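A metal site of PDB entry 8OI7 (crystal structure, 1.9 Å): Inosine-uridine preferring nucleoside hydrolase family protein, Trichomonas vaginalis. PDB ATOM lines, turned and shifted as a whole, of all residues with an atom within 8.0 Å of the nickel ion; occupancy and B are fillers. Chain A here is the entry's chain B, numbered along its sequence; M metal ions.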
ATOM      1  N   ASN A  39       6.383  25.208   3.646  1.00  0.00           N
ATOM      2  CA  ASN A  39       7.059  25.784   2.487  1.00  0.00           C
ATOM      3  C   ASN A  39       6.480  25.224   1.189  1.00  0.00           C
ATOM      4  O   ASN A  39       6.656  25.837   0.137  1.00  0.00           O
ATOM      5  CB  ASN A  39       8.552  25.492   2.492  1.00  0.00           C
ATOM      6  CG  ASN A  39       9.342  26.459   3.346  1.00  0.00           C
ATOM      7  OD1 ASN A  39      10.078  26.045   4.244  1.00  0.00           O
ATOM      8  ND2 ASN A  39       9.210  27.744   3.068  1.00  0.00           N
ATOM      9  N   GLN A  40       5.874  24.037   1.279  1.00  0.00           N
ATOM     10  CA  GLN A  40       5.115  23.441   0.189  1.00  0.00           C
ATOM     11  C   GLN A  40       3.681  23.185   0.634  1.00  0.00           C
ATOM     12  O   GLN A  40       3.368  23.177   1.832  1.00  0.00           O
ATOM     13  CB  GLN A  40       5.762  22.135  -0.304  1.00  0.00           C
ATOM     14  CG  GLN A  40       7.182  22.276  -0.859  1.00  0.00           C
ATOM     15  CD  GLN A  40       7.377  23.329  -1.927  1.00  0.00           C
ATOM     16  OE1 GLN A  40       6.564  23.530  -2.835  1.00  0.00           O
ATOM     17  NE2 GLN A  40       8.495  24.034  -1.837  1.00  0.00           N
ATOM     18  N   LYS A  44       1.479  18.233  -1.037  1.00  0.00           N
ATOM     19  CA  LYS A  44       2.848  17.751  -1.185  1.00  0.00           C
ATOM     20  C   LYS A  44       3.334  17.118   0.110  1.00  0.00           C
ATOM     21  O   LYS A  44       3.988  16.073   0.063  1.00  0.00           O
ATOM     22  CB  LYS A  44       3.764  18.876  -1.685  1.00  0.00           C
ATOM     23  CG  LYS A  44       3.630  19.159  -3.175  1.00  0.00           C
ATOM     24  CD  LYS A  44       4.733  20.007  -3.779  1.00  0.00           C
ATOM     25  CE  LYS A  44       4.282  20.670  -5.057  1.00  0.00           C
ATOM     26  NZ  LYS A  44       5.415  21.186  -5.870  1.00  0.00           N
ATOM     27  N   VAL A  77       2.600  30.393   2.964  1.00  0.00           N
ATOM     28  CA  VAL A  77       3.897  30.777   2.403  1.00  0.00           C
ATOM     29  C   VAL A  77       4.384  29.691   1.442  1.00  0.00           C
ATOM     30  O   VAL A  77       5.536  29.750   1.015  1.00  0.00           O
ATOM     31  CB  VAL A  77       4.944  31.070   3.499  1.00  0.00           C
ATOM     32  CG1 VAL A  77       4.566  32.303   4.322  1.00  0.00           C
ATOM     33  CG2 VAL A  77       5.195  29.870   4.386  1.00  0.00           C
ATOM     34  N   ALA A  78       3.492  28.743   1.100  1.00  0.00           N
ATOM     35  CA  ALA A  78       3.842  27.635   0.235  1.00  0.00           C
ATOM     36  C   ALA A  78       4.176  28.168  -1.154  1.00  0.00           C
ATOM     37  O   ALA A  78       3.489  29.056  -1.652  1.00  0.00           O
ATOM     38  CB  ALA A  78       2.708  26.629   0.171  1.00  0.00           C
ATOM     39  N   CYS A  79       5.249  27.635  -1.763  1.00  0.00           N
ATOM     40  CA  CYS A  79       5.527  27.908  -3.159  1.00  0.00           C
ATOM     41  C   CYS A  79       4.333  27.465  -3.997  1.00  0.00           C
ATOM     42  O   CYS A  79       3.609  26.548  -3.609  1.00  0.00           O
ATOM     43  CB  CYS A  79       6.783  27.191  -3.625  1.00  0.00           C
ATOM     44  SG  CYS A  79       8.311  27.951  -3.013  1.00  0.00           S
ATOM     45  N   PRO A  80       4.085  28.101  -5.167  1.00  0.00           N
ATOM     46  CA  PRO A  80       3.103  27.575  -6.120  1.00  0.00           C
ATOM     47  C   PRO A  80       3.651  26.293  -6.731  1.00  0.00           C
ATOM     48  O   PRO A  80       4.872  26.135  -6.845  1.00  0.00           O
ATOM     49  CB  PRO A  80       2.941  28.710  -7.150  1.00  0.00           C
ATOM     50  CG  PRO A  80       4.264  29.445  -7.087  1.00  0.00           C
ATOM     51  CD  PRO A  80       4.719  29.332  -5.647  1.00  0.00           C
ATOM     52  N   GLU A  81       2.749  25.380  -7.103  1.00  0.00           N
ATOM     53  CA  GLU A  81       3.131  24.047  -7.553  1.00  0.00           C
ATOM     54  C   GLU A  81       3.906  24.122  -8.856  1.00  0.00           C
ATOM     55  O   GLU A  81       4.729  23.255  -9.133  1.00  0.00           O
ATOM     56  CB  GLU A  81       1.896  23.140  -7.650  1.00  0.00           C
ATOM     57  CG  GLU A  81       1.655  22.322  -6.382  1.00  0.00           C
ATOM     58  CD  GLU A  81       0.224  21.941  -6.041  1.00  0.00           C
ATOM     59  OE1 GLU A  81       0.059  21.014  -5.225  1.00  0.00           O
ATOM     60  OE2 GLU A  81      -0.711  22.594  -6.560  1.00  0.00           O
ATOM     61  N   ILE A  82       3.680  25.199  -9.631  1.00  0.00           N
ATOM     62  CA  ILE A  82       4.353  25.395 -10.909  1.00  0.00           C
ATOM     63  C   ILE A  82       5.838  25.769 -10.718  1.00  0.00           C
ATOM     64  O   ILE A  82       6.542  25.904 -11.711  1.00  0.00           O
ATOM     65  CB  ILE A  82       3.587  26.413 -11.784  1.00  0.00           C
ATOM     66  CG1 ILE A  82       3.538  27.828 -11.177  1.00  0.00           C
ATOM     67  CG2 ILE A  82       2.196  25.883 -12.096  1.00  0.00           C
ATOM     68  CD1 ILE A  82       4.813  28.629 -11.361  1.00  0.00           C
ATOM     69  N   HIS A  83       6.313  25.959  -9.478  1.00  0.00           N
ATOM     70  CA  HIS A  83       7.749  25.935  -9.190  1.00  0.00           C
ATOM     71  C   HIS A  83       8.326  24.532  -9.337  1.00  0.00           C
ATOM     72  O   HIS A  83       9.518  24.389  -9.591  1.00  0.00           O
ATOM     73  CB  HIS A  83       8.063  26.433  -7.780  1.00  0.00           C
ATOM     74  CG  HIS A  83       8.080  27.920  -7.615  1.00  0.00           C
ATOM     75  ND1 HIS A  83       8.629  28.500  -6.500  1.00  0.00           N
ATOM     76  CD2 HIS A  83       7.677  28.921  -8.399  1.00  0.00           C
ATOM     77  CE1 HIS A  83       8.534  29.817  -6.605  1.00  0.00           C
ATOM     78  NE2 HIS A  83       7.955  30.097  -7.757  1.00  0.00           N
ATOM     79  N   GLY A  84       7.498  23.508  -9.099  1.00  0.00           N
ATOM     80  CA  GLY A  84       7.881  22.124  -9.310  1.00  0.00           C
ATOM     81  C   GLY A  84       8.863  21.608  -8.252  1.00  0.00           C
ATOM     82  O   GLY A  84       9.683  20.750  -8.552  1.00  0.00           O
ATOM     83  N   GLU A  85       8.741  22.125  -7.022  1.00  0.00           N
ATOM     84  CA  GLU A  85       9.591  21.730  -5.911  1.00  0.00           C
ATOM     85  C   GLU A  85       8.874  20.694  -5.051  1.00  0.00           C
ATOM     86  O   GLU A  85       7.742  20.915  -4.614  1.00  0.00           O
ATOM     87  CB  GLU A  85       9.985  22.973  -5.107  1.00  0.00           C
ATOM     88  CG  GLU A  85      10.769  23.977  -5.932  1.00  0.00           C
ATOM     89  CD  GLU A  85      10.795  25.429  -5.470  1.00  0.00           C
ATOM     90  OE1 GLU A  85       9.832  25.884  -4.813  1.00  0.00           O
ATOM     91  OE2 GLU A  85      11.785  26.104  -5.767  1.00  0.00           O
HETATM   92 NI    NI M   1       9.628  27.804  -4.955  1.00  0.00          NI
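The backbone NH of Cys 79 is in hydrogen-bond range of the backbone carbonyl oxygen of Asn 39. The backbone carbonyl oxygen (O) of Glu 85 lies close to the side-chain amide oxygen (OE1) of Gln 40, at 3.4 Å. O of Glu 85 sits at hydrogen-bond distance from NZ of Lys 44 (2.7 Å).
Along chain A the residues within 4 Å of the nickel ion span positions 79 to 85.
The nickel ion is bound by the side-chain carboxylate (OE1) of Glu 85 (1.9 Å), a ring nitrogen (ND1) of His 83 (2.0 Å) and the side-chain sulfur (SG) of Cys 79 (2.4 Å). The nickel ion has three donor atoms within binding distance.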
